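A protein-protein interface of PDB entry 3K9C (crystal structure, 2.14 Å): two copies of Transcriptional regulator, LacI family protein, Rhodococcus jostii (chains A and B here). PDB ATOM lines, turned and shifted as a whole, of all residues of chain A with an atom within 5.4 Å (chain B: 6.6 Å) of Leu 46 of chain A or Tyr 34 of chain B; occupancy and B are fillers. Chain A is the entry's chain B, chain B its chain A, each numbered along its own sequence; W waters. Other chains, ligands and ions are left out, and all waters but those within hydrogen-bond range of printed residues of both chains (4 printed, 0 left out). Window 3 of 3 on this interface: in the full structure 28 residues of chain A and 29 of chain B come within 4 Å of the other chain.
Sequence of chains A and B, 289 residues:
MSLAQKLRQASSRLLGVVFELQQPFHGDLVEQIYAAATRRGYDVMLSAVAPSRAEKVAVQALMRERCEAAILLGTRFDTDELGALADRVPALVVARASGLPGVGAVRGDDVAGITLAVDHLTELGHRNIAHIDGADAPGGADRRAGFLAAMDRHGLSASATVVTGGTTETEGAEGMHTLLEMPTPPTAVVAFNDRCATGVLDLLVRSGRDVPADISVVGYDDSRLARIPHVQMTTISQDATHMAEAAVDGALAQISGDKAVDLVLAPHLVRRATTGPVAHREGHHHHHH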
ATOM      1  N   VAL A  17      -9.324  27.565 -30.581  1.00  0.00           N
ATOM      2  CA  VAL A  17      -8.820  28.917 -30.818  1.00  0.00           C
ATOM      3  C   VAL A  17      -7.647  29.264 -29.897  1.00  0.00           C
ATOM      4  O   VAL A  17      -7.794  29.293 -28.680  1.00  0.00           O
ATOM      5  CB  VAL A  17      -9.939  29.973 -30.607  1.00  0.00           C
ATOM      6  CG1 VAL A  17      -9.391  31.376 -30.855  1.00  0.00           C
ATOM      7  CG2 VAL A  17     -11.102  29.687 -31.533  1.00  0.00           C
ATOM      8  N   PHE A  19      -5.048  32.095 -28.620  1.00  0.00           N
ATOM      9  CA  PHE A  19      -4.964  33.564 -28.598  1.00  0.00           C
ATOM     10  C   PHE A  19      -4.121  34.087 -27.438  1.00  0.00           C
ATOM     11  O   PHE A  19      -3.925  33.394 -26.437  1.00  0.00           O
ATOM     12  CB  PHE A  19      -6.365  34.181 -28.489  1.00  0.00           C
ATOM     13  CG  PHE A  19      -6.918  34.165 -27.099  1.00  0.00           C
ATOM     14  CD1 PHE A  19      -7.005  35.337 -26.360  1.00  0.00           C
ATOM     15  CD2 PHE A  19      -7.331  32.973 -26.517  1.00  0.00           C
ATOM     16  CE1 PHE A  19      -7.497  35.323 -25.056  1.00  0.00           C
ATOM     17  CE2 PHE A  19      -7.820  32.945 -25.222  1.00  0.00           C
ATOM     18  CZ  PHE A  19      -7.906  34.120 -24.489  1.00  0.00           C
ATOM     19  N   VAL A  30     -11.719  37.128 -30.454  1.00  0.00           N
ATOM     20  CA  VAL A  30     -12.287  35.992 -29.725  1.00  0.00           C
ATOM     21  C   VAL A  30     -13.786  36.183 -29.499  1.00  0.00           C
ATOM     22  O   VAL A  30     -14.577  35.272 -29.746  1.00  0.00           O
ATOM     23  CB  VAL A  30     -11.611  35.788 -28.344  1.00  0.00           C
ATOM     24  CG1 VAL A  30     -12.486  34.901 -27.471  1.00  0.00           C
ATOM     25  CG2 VAL A  30     -10.225  35.144 -28.522  1.00  0.00           C
ATOM     26  N   TYR A  34     -16.574  33.568 -31.097  1.00  0.00           N
ATOM     27  CA  TYR A  34     -17.555  32.857 -30.292  1.00  0.00           C
ATOM     28  C   TYR A  34     -18.934  33.025 -30.927  1.00  0.00           C
ATOM     29  O   TYR A  34     -19.674  32.055 -31.090  1.00  0.00           O
ATOM     30  CB  TYR A  34     -17.608  33.435 -28.882  1.00  0.00           C
ATOM     31  CG  TYR A  34     -16.808  32.701 -27.827  1.00  0.00           C
ATOM     32  CD1 TYR A  34     -15.800  33.355 -27.127  1.00  0.00           C
ATOM     33  CD2 TYR A  34     -17.119  31.382 -27.464  1.00  0.00           C
ATOM     34  CE1 TYR A  34     -15.120  32.730 -26.079  1.00  0.00           C
ATOM     35  CE2 TYR A  34     -16.443  30.742 -26.417  1.00  0.00           C
ATOM     36  CZ  TYR A  34     -15.446  31.427 -25.728  1.00  0.00           C
ATOM     37  OH  TYR A  34     -14.783  30.842 -24.678  1.00  0.00           O
ATOM     38  N   VAL A  44     -16.677  26.776 -28.936  1.00  0.00           N
ATOM     39  CA  VAL A  44     -15.295  27.172 -29.061  1.00  0.00           C
ATOM     40  C   VAL A  44     -14.514  26.806 -27.828  1.00  0.00           C
ATOM     41  O   VAL A  44     -14.983  26.979 -26.703  1.00  0.00           O
ATOM     42  CB  VAL A  44     -15.168  28.692 -29.304  1.00  0.00           C
ATOM     43  CG1 VAL A  44     -13.714  29.125 -29.157  1.00  0.00           C
ATOM     44  CG2 VAL A  44     -15.671  29.037 -30.701  1.00  0.00           C
ATOM     45  N   MET A  45     -13.318  26.280 -28.053  1.00  0.00           N
ATOM     46  CA  MET A  45     -12.439  25.934 -26.956  1.00  0.00           C
ATOM     47  C   MET A  45     -11.222  26.850 -27.077  1.00  0.00           C
ATOM     48  O   MET A  45     -10.491  26.789 -28.057  1.00  0.00           O
ATOM     49  CB  MET A  45     -12.007  24.474 -27.049  1.00  0.00           C
ATOM     50  CG  MET A  45     -11.634  23.893 -25.709  1.00  0.00           C
ATOM     51  SD  MET A  45     -10.190  22.625 -25.889  1.00  0.00           S
ATOM     52  CE  MET A  45      -8.832  23.579 -24.874  1.00  0.00           C
ATOM     53  N   LEU A  46     -11.038  27.718 -26.093  1.00  0.00           N
ATOM     54  CA  LEU A  46      -9.909  28.634 -26.082  1.00  0.00           C
ATOM     55  C   LEU A  46      -8.733  27.965 -25.398  1.00  0.00           C
ATOM     56  O   LEU A  46      -8.913  27.137 -24.510  1.00  0.00           O
ATOM     57  CB  LEU A  46     -10.239  29.883 -25.274  1.00  0.00           C
ATOM     58  CG  LEU A  46     -11.475  30.702 -25.604  1.00  0.00           C
ATOM     59  CD1 LEU A  46     -11.714  31.708 -24.482  1.00  0.00           C
ATOM     60  CD2 LEU A  46     -11.280  31.379 -26.936  1.00  0.00           C
ATOM     61  N   SER A  47      -7.534  28.333 -25.829  1.00  0.00           N
ATOM     62  CA  SER A  47      -6.295  27.856 -25.232  1.00  0.00           C
ATOM     63  C   SER A  47      -5.470  29.126 -25.285  1.00  0.00           C
ATOM     64  O   SER A  47      -5.162  29.629 -26.372  1.00  0.00           O
ATOM     65  CB  SER A  47      -5.641  26.767 -26.071  1.00  0.00           C
ATOM     66  OG  SER A  47      -4.479  26.286 -25.413  1.00  0.00           O
ATOM     67  N   ALA A  48      -5.119  29.653 -24.117  1.00  0.00           N
ATOM     68  CA  ALA A  48      -4.395  30.912 -24.061  1.00  0.00           C
ATOM     69  C   ALA A  48      -2.877  30.858 -24.061  1.00  0.00           C
ATOM     70  O   ALA A  48      -2.263  29.944 -23.508  1.00  0.00           O
ATOM     71  CB  ALA A  48      -4.870  31.713 -22.853  1.00  0.00           C
ATOM     72  N   ARG A  53       3.167  30.726 -20.493  1.00  0.00           N
ATOM     73  CA  ARG A  53       2.536  29.612 -21.197  1.00  0.00           C
ATOM     74  C   ARG A  53       2.757  29.719 -22.697  1.00  0.00           C
ATOM     75  O   ARG A  53       1.967  30.340 -23.412  1.00  0.00           O
ATOM     76  CB  ARG A  53       1.032  29.533 -20.886  1.00  0.00           C
ATOM     77  CG  ARG A  53       0.505  28.098 -21.017  1.00  0.00           C
ATOM     78  CD  ARG A  53      -0.912  27.899 -20.502  1.00  0.00           C
ATOM     79  NE  ARG A  53      -1.876  28.046 -21.578  1.00  0.00           N
ATOM     80  CZ  ARG A  53      -2.599  27.059 -22.096  1.00  0.00           C
ATOM     81  NH1 ARG A  53      -2.486  25.824 -21.634  1.00  0.00           N
ATOM     82  NH2 ARG A  53      -3.424  27.313 -23.095  1.00  0.00           N
ATOM     83  N   LEU A  62      -4.811  22.027 -27.028  1.00  0.00           N
ATOM     84  CA  LEU A  62      -5.969  21.877 -27.905  1.00  0.00           C
ATOM     85  C   LEU A  62      -6.017  20.469 -28.478  1.00  0.00           C
ATOM     86  O   LEU A  62      -7.095  19.922 -28.724  1.00  0.00           O
ATOM     87  CB  LEU A  62      -5.915  22.866 -29.074  1.00  0.00           C
ATOM     88  CG  LEU A  62      -6.510  24.263 -28.902  1.00  0.00           C
ATOM     89  CD1 LEU A  62      -6.387  25.024 -30.217  1.00  0.00           C
ATOM     90  CD2 LEU A  62      -7.973  24.159 -28.495  1.00  0.00           C
ATOM     91  N   PHE B  19     -14.093  33.581 -17.049  1.00  0.00           N
ATOM     92  CA  PHE B  19     -13.417  34.853 -16.784  1.00  0.00           C
ATOM     93  C   PHE B  19     -13.896  35.932 -17.761  1.00  0.00           C
ATOM     94  O   PHE B  19     -14.535  35.625 -18.770  1.00  0.00           O
ATOM     95  CB  PHE B  19     -11.907  34.665 -16.937  1.00  0.00           C
ATOM     96  CG  PHE B  19     -11.455  34.619 -18.367  1.00  0.00           C
ATOM     97  CD1 PHE B  19     -10.668  35.644 -18.897  1.00  0.00           C
ATOM     98  CD2 PHE B  19     -11.866  33.587 -19.205  1.00  0.00           C
ATOM     99  CE1 PHE B  19     -10.304  35.641 -20.247  1.00  0.00           C
ATOM    100  CE2 PHE B  19     -11.508  33.576 -20.551  1.00  0.00           C
ATOM    101  CZ  PHE B  19     -10.727  34.604 -21.075  1.00  0.00           C
ATOM    102  N   LEU B  21     -13.138  38.463 -20.587  1.00  0.00           N
ATOM    103  CA  LEU B  21     -12.183  38.686 -21.663  1.00  0.00           C
ATOM    104  C   LEU B  21     -11.376  39.987 -21.602  1.00  0.00           C
ATOM    105  O   LEU B  21     -10.160  39.977 -21.798  1.00  0.00           O
ATOM    106  CB  LEU B  21     -12.917  38.597 -22.999  1.00  0.00           C
ATOM    107  CG  LEU B  21     -12.140  38.162 -24.238  1.00  0.00           C
ATOM    108  CD1 LEU B  21     -11.242  36.978 -23.904  1.00  0.00           C
ATOM    109  CD2 LEU B  21     -13.136  37.797 -25.341  1.00  0.00           C
ATOM    110  N   LEU B  29      -5.179  36.238 -13.172  1.00  0.00           N
ATOM    111  CA  LEU B  29      -5.714  35.043 -12.526  1.00  0.00           C
ATOM    112  C   LEU B  29      -5.711  33.825 -13.453  1.00  0.00           C
ATOM    113  O   LEU B  29      -5.274  32.738 -13.057  1.00  0.00           O
ATOM    114  CB  LEU B  29      -7.128  35.310 -11.999  1.00  0.00           C
ATOM    115  CG  LEU B  29      -7.183  36.189 -10.740  1.00  0.00           C
ATOM    116  CD1 LEU B  29      -8.631  36.503 -10.358  1.00  0.00           C
ATOM    117  CD2 LEU B  29      -6.469  35.478  -9.606  1.00  0.00           C
ATOM    118  N   VAL B  30      -6.174  34.009 -14.689  1.00  0.00           N
ATOM    119  CA  VAL B  30      -6.222  32.914 -15.645  1.00  0.00           C
ATOM    120  C   VAL B  30      -4.834  32.343 -15.911  1.00  0.00           C
ATOM    121  O   VAL B  30      -4.639  31.130 -15.851  1.00  0.00           O
ATOM    122  CB  VAL B  30      -6.879  33.354 -16.984  1.00  0.00           C
ATOM    123  CG1 VAL B  30      -6.650  32.295 -18.063  1.00  0.00           C
ATOM    124  CG2 VAL B  30      -8.371  33.555 -16.772  1.00  0.00           C
ATOM    125  N   GLU B  31      -3.874  33.210 -16.210  1.00  0.00           N
ATOM    126  CA  GLU B  31      -2.516  32.751 -16.458  1.00  0.00           C
ATOM    127  C   GLU B  31      -2.033  31.920 -15.267  1.00  0.00           C
ATOM    128  O   GLU B  31      -1.428  30.869 -15.442  1.00  0.00           O
ATOM    129  CB  GLU B  31      -1.566  33.940 -16.683  1.00  0.00           C
ATOM    130  CG  GLU B  31      -0.113  33.526 -16.879  1.00  0.00           C
ATOM    131  CD  GLU B  31       0.806  34.682 -17.260  1.00  0.00           C
ATOM    132  OE1 GLU B  31       0.333  35.841 -17.321  1.00  0.00           O
ATOM    133  OE2 GLU B  31       2.007  34.423 -17.496  1.00  0.00           O
ATOM    134  N   GLN B  32      -2.318  32.369 -14.051  1.00  0.00           N
ATOM    135  CA  GLN B  32      -1.864  31.622 -12.889  1.00  0.00           C
ATOM    136  C   GLN B  32      -2.668  30.342 -12.619  1.00  0.00           C
ATOM    137  O   GLN B  32      -2.140  29.388 -12.061  1.00  0.00           O
ATOM    138  CB  GLN B  32      -1.849  32.525 -11.651  1.00  0.00           C
ATOM    139  CG  GLN B  32      -0.791  33.622 -11.685  1.00  0.00           C
ATOM    140  CD  GLN B  32       0.609  33.089 -11.988  1.00  0.00           C
ATOM    141  OE1 GLN B  32       1.074  32.130 -11.368  1.00  0.00           O
ATOM    142  NE2 GLN B  32       1.280  33.710 -12.941  1.00  0.00           N
ATOM    143  N   ILE B  33      -3.940  30.319 -12.998  1.00  0.00           N
ATOM    144  CA  ILE B  33      -4.744  29.120 -12.804  1.00  0.00           C
ATOM    145  C   ILE B  33      -4.258  28.016 -13.759  1.00  0.00           C
ATOM    146  O   ILE B  33      -4.247  26.839 -13.397  1.00  0.00           O
ATOM    147  CB  ILE B  33      -6.244  29.400 -13.039  1.00  0.00           C
ATOM    148  CG1 ILE B  33      -6.772  30.321 -11.926  1.00  0.00           C
ATOM    149  CG2 ILE B  33      -7.022  28.086 -13.047  1.00  0.00           C
ATOM    150  CD1 ILE B  33      -8.180  30.860 -12.143  1.00  0.00           C
ATOM    151  N   TYR B  34      -3.854  28.400 -14.970  1.00  0.00           N
ATOM    152  CA  TYR B  34      -3.335  27.439 -15.951  1.00  0.00           C
ATOM    153  C   TYR B  34      -2.095  26.761 -15.359  1.00  0.00           C
ATOM    154  O   TYR B  34      -1.945  25.543 -15.439  1.00  0.00           O
ATOM    155  CB  TYR B  34      -2.900  28.142 -17.251  1.00  0.00           C
ATOM    156  CG  TYR B  34      -3.921  28.191 -18.374  1.00  0.00           C
ATOM    157  CD1 TYR B  34      -4.377  29.412 -18.872  1.00  0.00           C
ATOM    158  CD2 TYR B  34      -4.375  27.024 -18.986  1.00  0.00           C
ATOM    159  CE1 TYR B  34      -5.258  29.472 -19.961  1.00  0.00           C
ATOM    160  CE2 TYR B  34      -5.253  27.073 -20.073  1.00  0.00           C
ATOM    161  CZ  TYR B  34      -5.686  28.300 -20.558  1.00  0.00           C
ATOM    162  OH  TYR B  34      -6.512  28.355 -21.661  1.00  0.00           O
ATOM    163  N   ALA B  35      -1.198  27.563 -14.782  1.00  0.00           N
ATOM    164  CA  ALA B  35       0.032  27.022 -14.204  1.00  0.00           C
ATOM    165  C   ALA B  35      -0.246  26.150 -12.984  1.00  0.00           C
ATOM    166  O   ALA B  35       0.347  25.085 -12.836  1.00  0.00           O
ATOM    167  CB  ALA B  35       0.997  28.155 -13.835  1.00  0.00           C
ATOM    168  N   ALA B  36      -1.143  26.598 -12.111  1.00  0.00           N
ATOM    169  CA  ALA B  36      -1.471  25.822 -10.912  1.00  0.00           C
ATOM    170  C   ALA B  36      -2.139  24.504 -11.293  1.00  0.00           C
ATOM    171  O   ALA B  36      -1.797  23.438 -10.760  1.00  0.00           O
ATOM    172  CB  ALA B  36      -2.379  26.613 -10.010  1.00  0.00           C
ATOM    173  N   ALA B  37      -3.102  24.586 -12.207  1.00  0.00           N
ATOM    174  CA  ALA B  37      -3.819  23.412 -12.673  1.00  0.00           C
ATOM    175  C   ALA B  37      -2.844  22.395 -13.254  1.00  0.00           C
ATOM    176  O   ALA B  37      -2.940  21.205 -12.952  1.00  0.00           O
ATOM    177  CB  ALA B  37      -4.857  23.811 -13.718  1.00  0.00           C
ATOM    178  N   THR B  38      -1.908  22.853 -14.085  1.00  0.00           N
ATOM    179  CA  THR B  38      -0.933  21.941 -14.679  1.00  0.00           C
ATOM    180  C   THR B  38      -0.056  21.298 -13.596  1.00  0.00           C
ATOM    181  O   THR B  38       0.249  20.111 -13.672  1.00  0.00           O
ATOM    182  CB  THR B  38      -0.031  22.657 -15.726  1.00  0.00           C
ATOM    183  OG1 THR B  38      -0.837  23.118 -16.822  1.00  0.00           O
ATOM    184  CG2 THR B  38       1.036  21.699 -16.275  1.00  0.00           C
ATOM    185  N   ARG B  39       0.338  22.071 -12.589  1.00  0.00           N
ATOM    186  CA  ARG B  39       1.158  21.526 -11.509  1.00  0.00           C
ATOM    187  C   ARG B  39       0.407  20.430 -10.764  1.00  0.00           C
ATOM    188  O   ARG B  39       1.018  19.553 -10.160  1.00  0.00           O
ATOM    189  CB  ARG B  39       1.574  22.616 -10.507  1.00  0.00           C
ATOM    190  CG  ARG B  39       2.789  23.442 -10.934  1.00  0.00           C
ATOM    191  CD  ARG B  39       3.331  24.285  -9.775  1.00  0.00           C
ATOM    192  NE  ARG B  39       2.372  25.279  -9.293  1.00  0.00           N
ATOM    193  CZ  ARG B  39       2.220  26.500  -9.803  1.00  0.00           C
ATOM    194  NH1 ARG B  39       2.965  26.911 -10.822  1.00  0.00           N
ATOM    195  NH2 ARG B  39       1.321  27.318  -9.288  1.00  0.00           N
ATOM    196  N   TYR B  42      -3.986  18.851 -13.937  1.00  0.00           N
ATOM    197  CA  TYR B  42      -5.282  19.172 -14.525  1.00  0.00           C
ATOM    198  C   TYR B  42      -5.184  20.147 -15.683  1.00  0.00           C
ATOM    199  O   TYR B  42      -4.329  21.034 -15.704  1.00  0.00           O
ATOM    200  CB  TYR B  42      -6.219  19.800 -13.490  1.00  0.00           C
ATOM    201  CG  TYR B  42      -6.927  18.819 -12.588  1.00  0.00           C
ATOM    202  CD1 TYR B  42      -6.274  18.235 -11.501  1.00  0.00           C
ATOM    203  CD2 TYR B  42      -8.258  18.470 -12.827  1.00  0.00           C
ATOM    204  CE1 TYR B  42      -6.937  17.325 -10.674  1.00  0.00           C
ATOM    205  CE2 TYR B  42      -8.921  17.569 -12.013  1.00  0.00           C
ATOM    206  CZ  TYR B  42      -8.259  17.003 -10.941  1.00  0.00           C
ATOM    207  OH  TYR B  42      -8.931  16.125 -10.131  1.00  0.00           O
ATOM    208  N   ASP B  43      -6.070  19.977 -16.650  1.00  0.00           N
ATOM    209  CA  ASP B  43      -6.124  20.881 -17.779  1.00  0.00           C
ATOM    210  C   ASP B  43      -7.227  21.894 -17.470  1.00  0.00           C
ATOM    211  O   ASP B  43      -8.032  21.702 -16.557  1.00  0.00           O
ATOM    212  CB  ASP B  43      -6.425  20.121 -19.071  1.00  0.00           C
ATOM    213  CG  ASP B  43      -5.171  19.555 -19.718  1.00  0.00           C
ATOM    214  OD1 ASP B  43      -4.210  20.327 -19.934  1.00  0.00           O
ATOM    215  OD2 ASP B  43      -5.142  18.344 -20.022  1.00  0.00           O
ATOM    216  N   VAL B  44      -7.265  22.974 -18.230  1.00  0.00           N
ATOM    217  CA  VAL B  44      -8.251  24.011 -17.991  1.00  0.00           C
ATOM    218  C   VAL B  44      -9.091  24.284 -19.225  1.00  0.00           C
ATOM    219  O   VAL B  44      -8.577  24.289 -20.343  1.00  0.00           O
ATOM    220  CB  VAL B  44      -7.562  25.344 -17.569  1.00  0.00           C
ATOM    221  CG1 VAL B  44      -8.593  26.451 -17.438  1.00  0.00           C
ATOM    222  CG2 VAL B  44      -6.814  25.158 -16.251  1.00  0.00           C
ATOM    223  N   MET B  45     -10.389  24.484 -19.017  1.00  0.00           N
ATOM    224  CA  MET B  45     -11.278  24.835 -20.109  1.00  0.00           C
ATOM    225  C   MET B  45     -11.771  26.243 -19.791  1.00  0.00           C
ATOM    226  O   MET B  45     -12.454  26.452 -18.787  1.00  0.00           O
ATOM    227  CB  MET B  45     -12.486  23.898 -20.202  1.00  0.00           C
ATOM    228  CG  MET B  45     -13.218  24.069 -21.521  1.00  0.00           C
ATOM    229  SD  MET B  45     -15.100  23.616 -21.444  1.00  0.00           S
ATOM    230  CE  MET B  45     -15.816  25.271 -22.233  1.00  0.00           C
ATOM    231  N   LEU B  46     -11.395  27.207 -20.630  1.00  0.00           N
ATOM    232  CA  LEU B  46     -11.808  28.596 -20.457  1.00  0.00           C
ATOM    233  C   LEU B  46     -13.098  28.876 -21.218  1.00  0.00           C
ATOM    234  O   LEU B  46     -13.303  28.376 -22.315  1.00  0.00           O
ATOM    235  CB  LEU B  46     -10.740  29.550 -20.985  1.00  0.00           C
ATOM    236  CG  LEU B  46      -9.446  29.789 -20.221  1.00  0.00           C
ATOM    237  CD1 LEU B  46      -8.533  30.654 -21.084  1.00  0.00           C
ATOM    238  CD2 LEU B  46      -9.737  30.480 -18.902  1.00  0.00           C
ATOM    239  N   SER B  47     -13.965  29.679 -20.618  1.00  0.00           N
ATOM    240  CA  SER B  47     -15.216  30.068 -21.253  1.00  0.00           C
ATOM    241  C   SER B  47     -15.301  31.552 -20.930  1.00  0.00           C
ATOM    242  O   SER B  47     -15.517  31.936 -19.778  1.00  0.00           O
ATOM    243  CB  SER B  47     -16.399  29.317 -20.649  1.00  0.00           C
ATOM    244  OG  SER B  47     -17.594  29.689 -21.310  1.00  0.00           O
ATOM    245  N   ALA B  48     -15.112  32.371 -21.957  1.00  0.00           N
ATOM    246  CA  ALA B  48     -15.098  33.813 -21.801  1.00  0.00           C
ATOM    247  C   ALA B  48     -16.434  34.506 -21.694  1.00  0.00           C
ATOM    248  O   ALA B  48     -17.413  34.116 -22.333  1.00  0.00           O
ATOM    249  CB  ALA B  48     -14.301  34.440 -22.939  1.00  0.00           C
ATOM    250  N   ALA B 244      -4.835  32.051  -7.293  1.00  0.00           N
ATOM    251  CA  ALA B 244      -5.063  31.034  -8.309  1.00  0.00           C
ATOM    252  C   ALA B 244      -4.728  29.646  -7.778  1.00  0.00           C
ATOM    253  O   ALA B 244      -5.465  28.697  -8.011  1.00  0.00           O
ATOM    254  CB  ALA B 244      -4.225  31.333  -9.551  1.00  0.00           C
ATOM    255  N   VAL B 248      -7.533  26.682  -7.315  1.00  0.00           N
ATOM    256  CA  VAL B 248      -7.381  25.350  -7.900  1.00  0.00           C
ATOM    257  C   VAL B 248      -7.380  24.263  -6.826  1.00  0.00           C
ATOM    258  O   VAL B 248      -8.051  23.247  -6.973  1.00  0.00           O
ATOM    259  CB  VAL B 248      -6.066  25.249  -8.728  1.00  0.00           C
ATOM    260  CG1 VAL B 248      -5.789  23.811  -9.112  1.00  0.00           C
ATOM    261  CG2 VAL B 248      -6.180  26.084  -9.993  1.00  0.00           C
HETATM  262  O   HOH W   1      -8.312  26.449 -22.164  1.00  0.00           O
HETATM  263  O   HOH W   2      -5.959  25.169 -22.832  1.00  0.00           O
HETATM  264  O   HOH W   3     -14.623  28.097 -24.482  1.00  0.00           O
HETATM  265  O   HOH W   4      -0.640  25.408 -18.783  1.00  0.00           O
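Water W3 lies within hydrogen-bond range of O of Val 44 of chain A, O of Leu 46 of chain B and OH of Tyr 34 of chain A.
Water W1 lies within hydrogen-bond range of the backbone carbonyl oxygen of Leu 46 of chain A (2.5 Å), the side-chain hydroxyl of Tyr 34 of chain B (2.7 Å) and the backbone carbonyl oxygen of Val 44 of chain B (2.8 Å).
Water W4 lies within hydrogen-bond range of the side-chain hydroxyl of Thr 38 of chain B (3.0 Å) and the guanidinium group of Arg 53 of chain A (3.4 Å).
Water W2 lies within hydrogen-bond range of the side-chain hydroxyl (OG) of Ser 47 of chain A (3.2 Å), the guanidinium group (NH2) of Arg 53 of chain A (3.3 Å) and the side-chain hydroxyl (OH) of Tyr 34 of chain B (3.4 Å).
N of Phe 19 of chain B is in hydrogen-bond range of O of Ser 47 of chain B (3.5 Å).
OG1 of Thr 38 of chain B is in hydrogen-bond range of O of Tyr 34 of chain B (3.0 Å).
N of Ser 47 of chain A sits at hydrogen-bond distance from O of Val 17 of chain A (3.0 Å).
The backbone NH of Phe 19 of chain A is in hydrogen-bond range of the backbone carbonyl oxygen of Ser 47 of chain A (3.3 Å).
The side-chain hydroxyl (OG) of Ser 47 of chain A sits at hydrogen-bond distance from the guanidinium group (NH2) of Arg 53 of chain A.
NE of Arg 53 of chain A lies within hydrogen-bond range of O of Ala 48 of chain A (2.7 Å).
Of the printed residues of chain B, Tyr 34 of chain A touches Leu 46 (3.7 Å), Ser 47 (3.5 Å) and Ala 48 (3.1 Å).
Of chain B, only Tyr 34 (3.9 Å) comes within 4 Å of Leu 46 of chain A.
Printed residues of chain B within 4 Å of Ala 48 of chain A: Tyr 34 (3.1 Å).
Of the printed residues of chain B, Arg 53 of chain A touches Tyr 34 (3.3 Å).
Ile 33 of chain B touches none of the printed residues of chain A.
Of chain A, only Leu 46 (3.9 Å), Ser 47 (3.6 Å), Ala 48 (3.1 Å) and Arg 53 (3.3 Å) come within 4 Å of Tyr 34 of chain B.
Arg 39 of chain B touches none of the printed residues of chain A.
The nearest printed residue of chain B that does not touch Ser 47 of chain A is Leu 46 of chain B (5.4 Å).
The side-chain hydroxyl (OH) of Tyr 34 of chain B sits at hydrogen-bond distance from the backbone NH (N) of Ala 48 of chain A (3.1 Å).
N of Ala 48 of chain B lies within hydrogen-bond range of OH of Tyr 34 of chain A (3.1 Å).
Tyr 34 of chain A touches Leu 46 of chain B, and with the chains exchanged Leu 46 of chain A touches Tyr 34 of chain B.
Tyr 34 of chain A touches Ser 47 of chain B, and with the chains exchanged Ser 47 of chain A touches Tyr 34 of chain B.
Tyr 34 of chain A touches Ala 48 of chain B, and with the chains exchanged Ala 48 of chain A touches Tyr 34 of chain B.
8 positions are printed for both chains.
Of the 8 pairs that touch across the chains among the printed residues, 6 have their exchanged pair printed and touching as well.
Printed residues of chain B that touch a printed residue of chain A: Leu 21, Tyr 34, Leu 46, Ser 47 and Ala 48.
Hydrophobic or aromatic side chains of chain B that line the printed part of chain A: Leu 21, Tyr 34 and Ala 48.
Hydrophobic or aromatic side chains of chain A that line the printed part of chain B: Val 30, Tyr 34 and Ala 48.
Among the printed residues, 8 pairs touch across the chains.
Among the printed residues, no Asp or Glu carboxylate lies within 4 Å of a Lys or Arg side-chain nitrogen of the other chain.
Leu 21 of chain B touches Val 30 of chain A (CD2 to CG1, 3.7 Å).
Tyr 34 of chain A touches Leu 46 of chain B (OH to O, 3.7 Å).
CA of Ser 47 of chain B touches OH of Tyr 34 of chain A (3.5 Å).
Leu 46 of chain A touches Tyr 34 of chain B.
Ser 47 of chain A touches Tyr 34 of chain B (CA to OH, 3.6 Å).
CZ of Arg 53 of chain A touches CE2 of Tyr 34 of chain B (3.3 Å).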
